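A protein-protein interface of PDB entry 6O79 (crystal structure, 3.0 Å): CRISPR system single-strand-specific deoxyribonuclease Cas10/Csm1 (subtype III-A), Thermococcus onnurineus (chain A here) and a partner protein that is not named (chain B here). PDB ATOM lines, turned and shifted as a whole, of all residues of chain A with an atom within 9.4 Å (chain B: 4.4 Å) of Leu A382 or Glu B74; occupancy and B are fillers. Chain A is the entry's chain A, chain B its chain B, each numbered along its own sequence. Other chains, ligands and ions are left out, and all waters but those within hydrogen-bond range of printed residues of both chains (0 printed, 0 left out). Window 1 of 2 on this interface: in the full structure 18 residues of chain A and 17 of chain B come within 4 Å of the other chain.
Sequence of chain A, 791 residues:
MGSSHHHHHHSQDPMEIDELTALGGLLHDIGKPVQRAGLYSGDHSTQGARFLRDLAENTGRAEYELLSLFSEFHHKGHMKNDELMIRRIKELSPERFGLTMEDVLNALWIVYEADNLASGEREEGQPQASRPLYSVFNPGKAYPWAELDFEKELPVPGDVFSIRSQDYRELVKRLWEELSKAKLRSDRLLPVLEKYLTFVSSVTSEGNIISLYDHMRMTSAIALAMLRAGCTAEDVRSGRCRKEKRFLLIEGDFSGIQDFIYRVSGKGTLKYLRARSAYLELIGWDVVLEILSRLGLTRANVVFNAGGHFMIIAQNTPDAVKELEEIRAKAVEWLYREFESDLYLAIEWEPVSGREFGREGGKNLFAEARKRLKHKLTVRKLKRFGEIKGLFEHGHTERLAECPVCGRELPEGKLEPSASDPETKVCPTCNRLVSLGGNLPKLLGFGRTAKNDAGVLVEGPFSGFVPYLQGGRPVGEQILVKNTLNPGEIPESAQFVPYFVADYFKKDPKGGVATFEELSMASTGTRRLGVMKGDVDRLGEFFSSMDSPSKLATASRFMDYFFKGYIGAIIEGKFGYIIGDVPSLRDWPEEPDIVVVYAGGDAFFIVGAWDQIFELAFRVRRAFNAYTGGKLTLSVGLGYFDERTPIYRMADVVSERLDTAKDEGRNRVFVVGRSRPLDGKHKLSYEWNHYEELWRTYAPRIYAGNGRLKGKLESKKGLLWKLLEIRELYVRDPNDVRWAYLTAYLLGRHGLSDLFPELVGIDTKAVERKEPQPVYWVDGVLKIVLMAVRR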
ATOM      1  N   SER A 255       7.170  23.440  -7.804  1.00  0.00           N
ATOM      2  CA  SER A 255       6.672  22.043  -7.919  1.00  0.00           C
ATOM      3  C   SER A 255       6.841  21.554  -9.360  1.00  0.00           C
ATOM      4  O   SER A 255       6.823  22.395 -10.279  1.00  0.00           O
ATOM      5  CB  SER A 255       5.246  21.927  -7.451  1.00  0.00           C
ATOM      6  OG  SER A 255       4.339  22.080  -8.532  1.00  0.00           O
ATOM      7  N   TYR A 344       5.670  24.996 -11.994  1.00  0.00           N
ATOM      8  CA  TYR A 344       4.759  25.906 -11.252  1.00  0.00           C
ATOM      9  C   TYR A 344       5.462  26.405  -9.985  1.00  0.00           C
ATOM     10  O   TYR A 344       6.249  25.636  -9.399  1.00  0.00           O
ATOM     11  CB  TYR A 344       3.455  25.192 -10.894  1.00  0.00           C
ATOM     12  CG  TYR A 344       2.540  25.984  -9.995  1.00  0.00           C
ATOM     13  CD1 TYR A 344       2.052  27.217 -10.393  1.00  0.00           C
ATOM     14  CD2 TYR A 344       2.170  25.515  -8.745  1.00  0.00           C
ATOM     15  CE1 TYR A 344       1.215  27.963  -9.578  1.00  0.00           C
ATOM     16  CE2 TYR A 344       1.331  26.246  -7.917  1.00  0.00           C
ATOM     17  CZ  TYR A 344       0.852  27.475  -8.336  1.00  0.00           C
ATOM     18  OH  TYR A 344       0.031  28.212  -7.537  1.00  0.00           O
ATOM     19  N   ALA A 346       4.414  27.678  -6.320  1.00  0.00           N
ATOM     20  CA  ALA A 346       3.412  27.796  -5.237  1.00  0.00           C
ATOM     21  C   ALA A 346       3.937  28.769  -4.178  1.00  0.00           C
ATOM     22  O   ALA A 346       4.835  28.371  -3.415  1.00  0.00           O
ATOM     23  CB  ALA A 346       3.122  26.436  -4.647  1.00  0.00           C
ATOM     24  N   LYS A 374       2.698  25.698   5.752  1.00  0.00           N
ATOM     25  CA  LYS A 374       2.957  24.488   4.926  1.00  0.00           C
ATOM     26  C   LYS A 374       1.627  24.010   4.333  1.00  0.00           C
ATOM     27  O   LYS A 374       1.533  23.910   3.095  1.00  0.00           O
ATOM     28  CB  LYS A 374       3.633  23.384   5.746  1.00  0.00           C
ATOM     29  CG  LYS A 374       4.020  22.140   4.956  1.00  0.00           C
ATOM     30  CD  LYS A 374       5.124  22.373   3.936  1.00  0.00           C
ATOM     31  CE  LYS A 374       4.985  21.531   2.682  1.00  0.00           C
ATOM     32  NZ  LYS A 374       4.208  22.226   1.627  1.00  0.00           N
ATOM     33  N   HIS A 375       0.633  23.761   5.190  1.00  0.00           N
ATOM     34  CA  HIS A 375      -0.734  23.317   4.802  1.00  0.00           C
ATOM     35  C   HIS A 375      -1.303  24.251   3.725  1.00  0.00           C
ATOM     36  O   HIS A 375      -1.907  23.736   2.768  1.00  0.00           O
ATOM     37  CB  HIS A 375      -1.655  23.231   6.025  1.00  0.00           C
ATOM     38  CG  HIS A 375      -3.011  22.702   5.700  1.00  0.00           C
ATOM     39  ND1 HIS A 375      -4.060  23.529   5.347  1.00  0.00           N
ATOM     40  CD2 HIS A 375      -3.487  21.439   5.650  1.00  0.00           C
ATOM     41  CE1 HIS A 375      -5.129  22.799   5.106  1.00  0.00           C
ATOM     42  NE2 HIS A 375      -4.803  21.511   5.285  1.00  0.00           N
ATOM     43  N   LYS A 376      -1.125  25.569   3.880  1.00  0.00           N
ATOM     44  CA  LYS A 376      -1.547  26.584   2.877  1.00  0.00           C
ATOM     45  C   LYS A 376      -0.911  26.243   1.523  1.00  0.00           C
ATOM     46  O   LYS A 376      -1.637  26.284   0.509  1.00  0.00           O
ATOM     47  CB  LYS A 376      -1.154  28.005   3.296  1.00  0.00           C
ATOM     48  CG  LYS A 376      -2.193  28.778   4.099  1.00  0.00           C
ATOM     49  CD  LYS A 376      -2.079  30.279   3.897  1.00  0.00           C
ATOM     50  CE  LYS A 376      -2.527  31.101   5.090  1.00  0.00           C
ATOM     51  NZ  LYS A 376      -4.000  31.248   5.137  1.00  0.00           N
ATOM     52  N   LEU A 377       0.387  25.914   1.516  1.00  0.00           N
ATOM     53  CA  LEU A 377       1.171  25.628   0.282  1.00  0.00           C
ATOM     54  C   LEU A 377       0.667  24.339  -0.372  1.00  0.00           C
ATOM     55  O   LEU A 377       0.351  24.385  -1.577  1.00  0.00           O
ATOM     56  CB  LEU A 377       2.660  25.523   0.618  1.00  0.00           C
ATOM     57  CG  LEU A 377       3.364  26.848   0.893  1.00  0.00           C
ATOM     58  CD1 LEU A 377       4.685  26.615   1.601  1.00  0.00           C
ATOM     59  CD2 LEU A 377       3.580  27.632  -0.393  1.00  0.00           C
ATOM     60  N   THR A 378       0.594  23.238   0.385  1.00  0.00           N
ATOM     61  CA  THR A 378       0.070  21.932  -0.102  1.00  0.00           C
ATOM     62  C   THR A 378      -1.251  22.180  -0.843  1.00  0.00           C
ATOM     63  O   THR A 378      -1.378  21.697  -1.981  1.00  0.00           O
ATOM     64  CB  THR A 378      -0.104  20.908   1.028  1.00  0.00           C
ATOM     65  OG1 THR A 378      -0.942  21.479   2.032  1.00  0.00           O
ATOM     66  CG2 THR A 378       1.209  20.469   1.640  1.00  0.00           C
ATOM     67  N   VAL A 379      -2.170  22.938  -0.234  1.00  0.00           N
ATOM     68  CA  VAL A 379      -3.492  23.307  -0.826  1.00  0.00           C
ATOM     69  C   VAL A 379      -3.248  24.020  -2.162  1.00  0.00           C
ATOM     70  O   VAL A 379      -3.921  23.664  -3.147  1.00  0.00           O
ATOM     71  CB  VAL A 379      -4.336  24.166   0.139  1.00  0.00           C
ATOM     72  CG1 VAL A 379      -5.542  24.796  -0.543  1.00  0.00           C
ATOM     73  CG2 VAL A 379      -4.784  23.368   1.353  1.00  0.00           C
ATOM     74  N   ARG A 380      -2.316  24.977  -2.202  1.00  0.00           N
ATOM     75  CA  ARG A 380      -2.032  25.787  -3.417  1.00  0.00           C
ATOM     76  C   ARG A 380      -1.475  24.880  -4.524  1.00  0.00           C
ATOM     77  O   ARG A 380      -1.778  25.151  -5.702  1.00  0.00           O
ATOM     78  CB  ARG A 380      -1.087  26.952  -3.096  1.00  0.00           C
ATOM     79  CG  ARG A 380      -0.716  27.819  -4.293  1.00  0.00           C
ATOM     80  CD  ARG A 380      -1.900  28.323  -5.101  1.00  0.00           C
ATOM     81  NE  ARG A 380      -2.554  29.482  -4.513  1.00  0.00           N
ATOM     82  CZ  ARG A 380      -3.627  30.087  -5.020  1.00  0.00           C
ATOM     83  NH1 ARG A 380      -4.185  29.641  -6.135  1.00  0.00           N
ATOM     84  NH2 ARG A 380      -4.142  31.138  -4.406  1.00  0.00           N
ATOM     85  N   LYS A 381      -0.721  23.833  -4.166  1.00  0.00           N
ATOM     86  CA  LYS A 381      -0.098  22.884  -5.133  1.00  0.00           C
ATOM     87  C   LYS A 381      -1.161  21.971  -5.762  1.00  0.00           C
ATOM     88  O   LYS A 381      -0.856  21.367  -6.808  1.00  0.00           O
ATOM     89  CB  LYS A 381       0.985  22.038  -4.459  1.00  0.00           C
ATOM     90  CG  LYS A 381       2.243  22.793  -4.055  1.00  0.00           C
ATOM     91  CD  LYS A 381       3.370  21.870  -3.643  1.00  0.00           C
ATOM     92  CE  LYS A 381       4.194  22.406  -2.494  1.00  0.00           C
ATOM     93  NZ  LYS A 381       5.219  21.426  -2.068  1.00  0.00           N
ATOM     94  N   LEU A 382      -2.345  21.858  -5.146  1.00  0.00           N
ATOM     95  CA  LEU A 382      -3.527  21.150  -5.713  1.00  0.00           C
ATOM     96  C   LEU A 382      -4.415  22.155  -6.461  1.00  0.00           C
ATOM     97  O   LEU A 382      -5.567  21.799  -6.774  1.00  0.00           O
ATOM     98  CB  LEU A 382      -4.306  20.469  -4.582  1.00  0.00           C
ATOM     99  CG  LEU A 382      -3.521  19.465  -3.737  1.00  0.00           C
ATOM    100  CD1 LEU A 382      -4.337  19.025  -2.531  1.00  0.00           C
ATOM    101  CD2 LEU A 382      -3.098  18.257  -4.558  1.00  0.00           C
ATOM    102  N   LYS A 383      -3.903  23.364  -6.722  1.00  0.00           N
ATOM    103  CA  LYS A 383      -4.601  24.446  -7.469  1.00  0.00           C
ATOM    104  C   LYS A 383      -3.603  25.102  -8.433  1.00  0.00           C
ATOM    105  O   LYS A 383      -3.645  26.340  -8.577  1.00  0.00           O
ATOM    106  CB  LYS A 383      -5.196  25.470  -6.495  1.00  0.00           C
ATOM    107  CG  LYS A 383      -6.162  24.907  -5.458  1.00  0.00           C
ATOM    108  CD  LYS A 383      -6.480  25.868  -4.329  1.00  0.00           C
ATOM    109  CE  LYS A 383      -7.505  26.921  -4.701  1.00  0.00           C
ATOM    110  NZ  LYS A 383      -8.886  26.477  -4.396  1.00  0.00           N
ATOM    111  N   ARG A 384      -2.747  24.293  -9.070  1.00  0.00           N
ATOM    112  CA  ARG A 384      -1.645  24.753  -9.959  1.00  0.00           C
ATOM    113  C   ARG A 384      -2.222  25.622 -11.080  1.00  0.00           C
ATOM    114  O   ARG A 384      -3.043  25.106 -11.861  1.00  0.00           O
ATOM    115  CB  ARG A 384      -0.880  23.565 -10.555  1.00  0.00           C
ATOM    116  CG  ARG A 384      -0.043  22.796  -9.543  1.00  0.00           C
ATOM    117  CD  ARG A 384       0.777  21.677 -10.161  1.00  0.00           C
ATOM    118  NE  ARG A 384       1.820  22.162 -11.057  1.00  0.00           N
ATOM    119  CZ  ARG A 384       2.746  21.398 -11.636  1.00  0.00           C
ATOM    120  NH1 ARG A 384       2.777  20.093 -11.420  1.00  0.00           N
ATOM    121  NH2 ARG A 384       3.646  21.946 -12.434  1.00  0.00           N
ATOM    122  N   PHE A 385      -1.810  26.892 -11.128  1.00  0.00           N
ATOM    123  CA  PHE A 385      -2.134  27.887 -12.187  1.00  0.00           C
ATOM    124  C   PHE A 385      -3.564  28.418 -12.013  1.00  0.00           C
ATOM    125  O   PHE A 385      -4.099  28.993 -12.982  1.00  0.00           O
ATOM    126  CB  PHE A 385      -1.918  27.290 -13.581  1.00  0.00           C
ATOM    127  CG  PHE A 385      -0.503  26.856 -13.868  1.00  0.00           C
ATOM    128  CD1 PHE A 385       0.507  27.793 -14.011  1.00  0.00           C
ATOM    129  CD2 PHE A 385      -0.181  25.515 -14.013  1.00  0.00           C
ATOM    130  CE1 PHE A 385       1.808  27.401 -14.286  1.00  0.00           C
ATOM    131  CE2 PHE A 385       1.121  25.122 -14.286  1.00  0.00           C
ATOM    132  CZ  PHE A 385       2.113  26.066 -14.424  1.00  0.00           C
ATOM    133  N   GLY A 386      -4.143  28.280 -10.814  1.00  0.00           N
ATOM    134  CA  GLY A 386      -5.442  28.882 -10.449  1.00  0.00           C
ATOM    135  C   GLY A 386      -5.428  30.393 -10.623  1.00  0.00           C
ATOM    136  O   GLY A 386      -6.519  30.985 -10.744  1.00  0.00           O
ATOM    137  N   GLU A 387      -4.230  30.988 -10.673  1.00  0.00           N
ATOM    138  CA  GLU A 387      -3.983  32.448 -10.823  1.00  0.00           C
ATOM    139  C   GLU A 387      -4.130  32.867 -12.296  1.00  0.00           C
ATOM    140  O   GLU A 387      -3.802  34.031 -12.611  1.00  0.00           O
ATOM    141  CB  GLU A 387      -2.586  32.787 -10.288  1.00  0.00           C
ATOM    142  CG  GLU A 387      -2.338  32.313  -8.861  1.00  0.00           C
ATOM    143  CD  GLU A 387      -1.577  31.002  -8.701  1.00  0.00           C
ATOM    144  OE1 GLU A 387      -0.776  30.902  -7.748  1.00  0.00           O
ATOM    145  OE2 GLU A 387      -1.788  30.077  -9.515  1.00  0.00           O
ATOM    146  N   LEU A 391      -7.229  29.657 -18.058  1.00  0.00           N
ATOM    147  CA  LEU A 391      -6.647  28.287 -18.056  1.00  0.00           C
ATOM    148  C   LEU A 391      -7.676  27.283 -18.594  1.00  0.00           C
ATOM    149  O   LEU A 391      -7.252  26.253 -19.154  1.00  0.00           O
ATOM    150  CB  LEU A 391      -6.216  27.928 -16.628  1.00  0.00           C
ATOM    151  CG  LEU A 391      -5.714  26.499 -16.412  1.00  0.00           C
ATOM    152  CD1 LEU A 391      -4.498  26.203 -17.277  1.00  0.00           C
ATOM    153  CD2 LEU A 391      -5.394  26.257 -14.946  1.00  0.00           C
ATOM    154  N   PHE A 392      -8.971  27.572 -18.424  1.00  0.00           N
ATOM    155  CA  PHE A 392     -10.095  26.659 -18.758  1.00  0.00           C
ATOM    156  C   PHE A 392     -10.949  27.278 -19.873  1.00  0.00           C
ATOM    157  O   PHE A 392     -12.176  27.425 -19.692  1.00  0.00           O
ATOM    158  CB  PHE A 392     -10.890  26.346 -17.488  1.00  0.00           C
ATOM    159  CG  PHE A 392     -10.049  25.813 -16.353  1.00  0.00           C
ATOM    160  CD1 PHE A 392      -9.235  24.704 -16.537  1.00  0.00           C
ATOM    161  CD2 PHE A 392     -10.067  26.416 -15.104  1.00  0.00           C
ATOM    162  CE1 PHE A 392      -8.464  24.209 -15.495  1.00  0.00           C
ATOM    163  CE2 PHE A 392      -9.292  25.921 -14.066  1.00  0.00           C
ATOM    164  CZ  PHE A 392      -8.493  24.820 -14.263  1.00  0.00           C
ATOM    165  N   LYS B  69      -7.954   7.787  -5.698  1.00  0.00           N
ATOM    166  CA  LYS B  69      -7.828   8.553  -4.429  1.00  0.00           C
ATOM    167  C   LYS B  69      -8.350   9.965  -4.673  1.00  0.00           C
ATOM    168  O   LYS B  69      -7.793  10.692  -5.493  1.00  0.00           O
ATOM    169  CB  LYS B  69      -6.362   8.580  -3.979  1.00  0.00           C
ATOM    170  CG  LYS B  69      -6.055   9.395  -2.729  1.00  0.00           C
ATOM    171  CD  LYS B  69      -4.578   9.709  -2.587  1.00  0.00           C
ATOM    172  CE  LYS B  69      -4.226  10.395  -1.283  1.00  0.00           C
ATOM    173  NZ  LYS B  69      -4.268   9.458  -0.135  1.00  0.00           N
ATOM    174  N   LEU B  71      -8.609  13.812  -4.257  1.00  0.00           N
ATOM    175  CA  LEU B  71      -7.651  14.862  -3.811  1.00  0.00           C
ATOM    176  C   LEU B  71      -8.190  15.578  -2.564  1.00  0.00           C
ATOM    177  O   LEU B  71      -7.416  16.328  -1.945  1.00  0.00           O
ATOM    178  CB  LEU B  71      -7.411  15.859  -4.951  1.00  0.00           C
ATOM    179  CG  LEU B  71      -6.749  15.300  -6.212  1.00  0.00           C
ATOM    180  CD1 LEU B  71      -6.467  16.414  -7.209  1.00  0.00           C
ATOM    181  CD2 LEU B  71      -5.464  14.553  -5.888  1.00  0.00           C
ATOM    182  N   SER B  72      -9.463  15.353  -2.212  1.00  0.00           N
ATOM    183  CA  SER B  72     -10.144  15.899  -1.008  1.00  0.00           C
ATOM    184  C   SER B  72      -9.362  15.569   0.271  1.00  0.00           C
ATOM    185  O   SER B  72      -9.391  16.400   1.200  1.00  0.00           O
ATOM    186  CB  SER B  72     -11.562  15.385  -0.911  1.00  0.00           C
ATOM    187  OG  SER B  72     -11.584  13.982  -0.676  1.00  0.00           O
ATOM    188  N   VAL B  73      -8.710  14.401   0.321  1.00  0.00           N
ATOM    189  CA  VAL B  73      -8.032  13.859   1.539  1.00  0.00           C
ATOM    190  C   VAL B  73      -6.630  14.467   1.677  1.00  0.00           C
ATOM    191  O   VAL B  73      -6.201  14.651   2.830  1.00  0.00           O
ATOM    192  CB  VAL B  73      -7.971  12.317   1.535  1.00  0.00           C
ATOM    193  CG1 VAL B  73      -9.352  11.697   1.402  1.00  0.00           C
ATOM    194  CG2 VAL B  73      -7.033  11.769   0.469  1.00  0.00           C
ATOM    195  N   GLU B  74      -5.955  14.768   0.558  1.00  0.00           N
ATOM    196  CA  GLU B  74      -4.534  15.222   0.523  1.00  0.00           C
ATOM    197  C   GLU B  74      -4.302  16.292   1.590  1.00  0.00           C
ATOM    198  O   GLU B  74      -3.349  16.184   2.358  1.00  0.00           O
ATOM    199  CB  GLU B  74      -4.132  15.746  -0.861  1.00  0.00           C
ATOM    200  CG  GLU B  74      -4.197  14.709  -1.972  1.00  0.00           C
ATOM    201  CD  GLU B  74      -3.086  13.674  -1.988  1.00  0.00           C
ATOM    202  OE1 GLU B  74      -2.253  13.680  -1.059  1.00  0.00           O
ATOM    203  OE2 GLU B  74      -3.057  12.861  -2.933  1.00  0.00           O
ATOM    204  N   PRO B  75      -5.143  17.351   1.685  1.00  0.00           N
ATOM    205  CA  PRO B  75      -4.988  18.361   2.734  1.00  0.00           C
ATOM    206  C   PRO B  75      -5.296  17.845   4.151  1.00  0.00           C
ATOM    207  O   PRO B  75      -4.611  18.241   5.075  1.00  0.00           O
ATOM    208  CB  PRO B  75      -6.002  19.459   2.360  1.00  0.00           C
ATOM    209  CG  PRO B  75      -6.390  19.165   0.925  1.00  0.00           C
ATOM    210  CD  PRO B  75      -6.264  17.665   0.787  1.00  0.00           C
ATOM    211  N   ALA B  76      -6.300  16.971   4.278  1.00  0.00           N
ATOM    212  CA  ALA B  76      -6.926  16.554   5.557  1.00  0.00           C
ATOM    213  C   ALA B  76      -6.131  15.440   6.254  1.00  0.00           C
ATOM    214  O   ALA B  76      -6.520  15.080   7.383  1.00  0.00           O
ATOM    215  CB  ALA B  76      -8.344  16.108   5.298  1.00  0.00           C
ATOM    216  N   LEU B  77      -5.062  14.923   5.630  1.00  0.00           N
ATOM    217  CA  LEU B  77      -4.307  13.719   6.090  1.00  0.00           C
ATOM    218  C   LEU B  77      -4.011  13.801   7.595  1.00  0.00           C
ATOM    219  O   LEU B  77      -4.023  12.737   8.250  1.00  0.00           O
ATOM    220  CB  LEU B  77      -3.008  13.592   5.286  1.00  0.00           C
ATOM    221  CG  LEU B  77      -3.166  13.156   3.828  1.00  0.00           C
ATOM    222  CD1 LEU B  77      -1.893  13.424   3.039  1.00  0.00           C
ATOM    223  CD2 LEU B  77      -3.554  11.688   3.730  1.00  0.00           C
ATOM    224  N   ARG B  97      -0.036   9.995   0.065  1.00  0.00           N
ATOM    225  CA  ARG B  97       0.136  11.054  -0.967  1.00  0.00           C
ATOM    226  C   ARG B  97       0.542  10.398  -2.295  1.00  0.00           C
ATOM    227  O   ARG B  97      -0.024  10.787  -3.334  1.00  0.00           O
ATOM    228  CB  ARG B  97       1.166  12.091  -0.504  1.00  0.00           C
ATOM    229  CG  ARG B  97       1.239  13.345  -1.365  1.00  0.00           C
ATOM    230  CD  ARG B  97       2.246  14.347  -0.828  1.00  0.00           C
ATOM    231  NE  ARG B  97       1.959  14.752   0.545  1.00  0.00           N
ATOM    232  CZ  ARG B  97       1.123  15.724   0.910  1.00  0.00           C
ATOM    233  NH1 ARG B  97       0.950  15.993   2.194  1.00  0.00           N
ATOM    234  NH2 ARG B  97       0.460  16.425   0.004  1.00  0.00           N
ATOM    235  N   LEU B 226     -10.069  21.482  -5.930  1.00  0.00           N
ATOM    236  CA  LEU B 226      -8.718  20.856  -5.916  1.00  0.00           C
ATOM    237  C   LEU B 226      -8.543  20.072  -7.220  1.00  0.00           C
ATOM    238  O   LEU B 226      -9.543  19.492  -7.686  1.00  0.00           O
ATOM    239  CB  LEU B 226      -8.599  19.927  -4.704  1.00  0.00           C
ATOM    240  CG  LEU B 226      -8.823  20.579  -3.342  1.00  0.00           C
ATOM    241  CD1 LEU B 226      -9.001  19.523  -2.262  1.00  0.00           C
ATOM    242  CD2 LEU B 226      -7.679  21.519  -2.993  1.00  0.00           C
ATOM    243  N   TRP B 227      -7.334  20.051  -7.791  1.00  0.00           N
ATOM    244  CA  TRP B 227      -7.085  19.375  -9.091  1.00  0.00           C
ATOM    245  C   TRP B 227      -5.597  19.124  -9.356  1.00  0.00           C
ATOM    246  O   TRP B 227      -4.745  19.823  -8.770  1.00  0.00           O
ATOM    247  CB  TRP B 227      -7.727  20.173 -10.233  1.00  0.00           C
ATOM    248  CG  TRP B 227      -7.006  21.427 -10.631  1.00  0.00           C
ATOM    249  CD1 TRP B 227      -6.067  21.552 -11.612  1.00  0.00           C
ATOM    250  CD2 TRP B 227      -7.202  22.749 -10.096  1.00  0.00           C
ATOM    251  NE1 TRP B 227      -5.654  22.853 -11.716  1.00  0.00           N
ATOM    252  CE2 TRP B 227      -6.332  23.611 -10.799  1.00  0.00           C
ATOM    253  CE3 TRP B 227      -8.013  23.287  -9.090  1.00  0.00           C
ATOM    254  CZ2 TRP B 227      -6.259  24.977 -10.529  1.00  0.00           C
ATOM    255  CZ3 TRP B 227      -7.944  24.639  -8.829  1.00  0.00           C
ATOM    256  CH2 TRP B 227      -7.077  25.471  -9.539  1.00  0.00           C
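The backbone carbonyl oxygen (O) of His A375 lies within hydrogen-bond range of the side-chain hydroxyl (OG1) of Thr A378 (2.6 Å).
A ring nitrogen (NE2) of His A375 sits at hydrogen-bond distance from the backbone carbonyl oxygen of Pro B75 (3.3 Å). The backbone carbonyl oxygen (O) of Leu A382 sits at hydrogen-bond distance from the backbone NH (N) of Trp B227 (2.7 Å). The indole nitrogen (NE1) of Trp B227 is in hydrogen-bond range of the backbone carbonyl oxygen (O) of Arg A384.
Among the printed residues, pairs that only touch across the chains: Lys A383 with Trp B227, Leu A382 with Leu B226, Leu A382 with Glu B74 and Gly A386 with Trp B227.
Of chain B, only Glu B74, Leu B226 and Trp B227 come within 4 Å of Leu A382. Of chain A, only Leu A382 (3.7 Å) comes within 4 Å of Glu B74. No residue of chain A comes within 4 Å of Leu B71. Trp B227 touches just these residues of chain A: Leu A382 (2.7 Å), Lys A383 (3.4 Å), Arg A384 (3.5 Å) and Gly A386 (3.9 Å). Printed residues of chain B within 4 Å of Lys A383: Trp B227. Of the printed residues of chain B, Gly A386 touches Trp B227. Val A379 touches none of the printed residues of chain B. Ala B76 touches none of the printed residues of chain A. The nearest residue of chain B that does not touch Leu A382 is Pro B75 (4.02 Å). The nearest residue of chain A that does not touch Glu B74 is Thr A378 (5.8 Å).
Of the 11 printed residues of chain B, 4 touch a printed residue of chain A. Hydrophobic or aromatic side chains of chain B within 4 Å of the printed part of chain A: Pro B75, Leu B226 and Trp B227. Of the 19 printed residues of chain A, 5 touch a printed residue of chain B. Printed residues of chain A that touch a printed residue of chain B: His A375, Leu A382, Lys A383, Arg A384 and Gly A386. Hydrophobic or aromatic side chains of chain A within 4 Å of the printed part of chain B: His A375 and Leu A382. Among the printed residues, no Asp or Glu carboxylate lies within 4 Å of a Lys or Arg side-chain nitrogen of the other chain.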
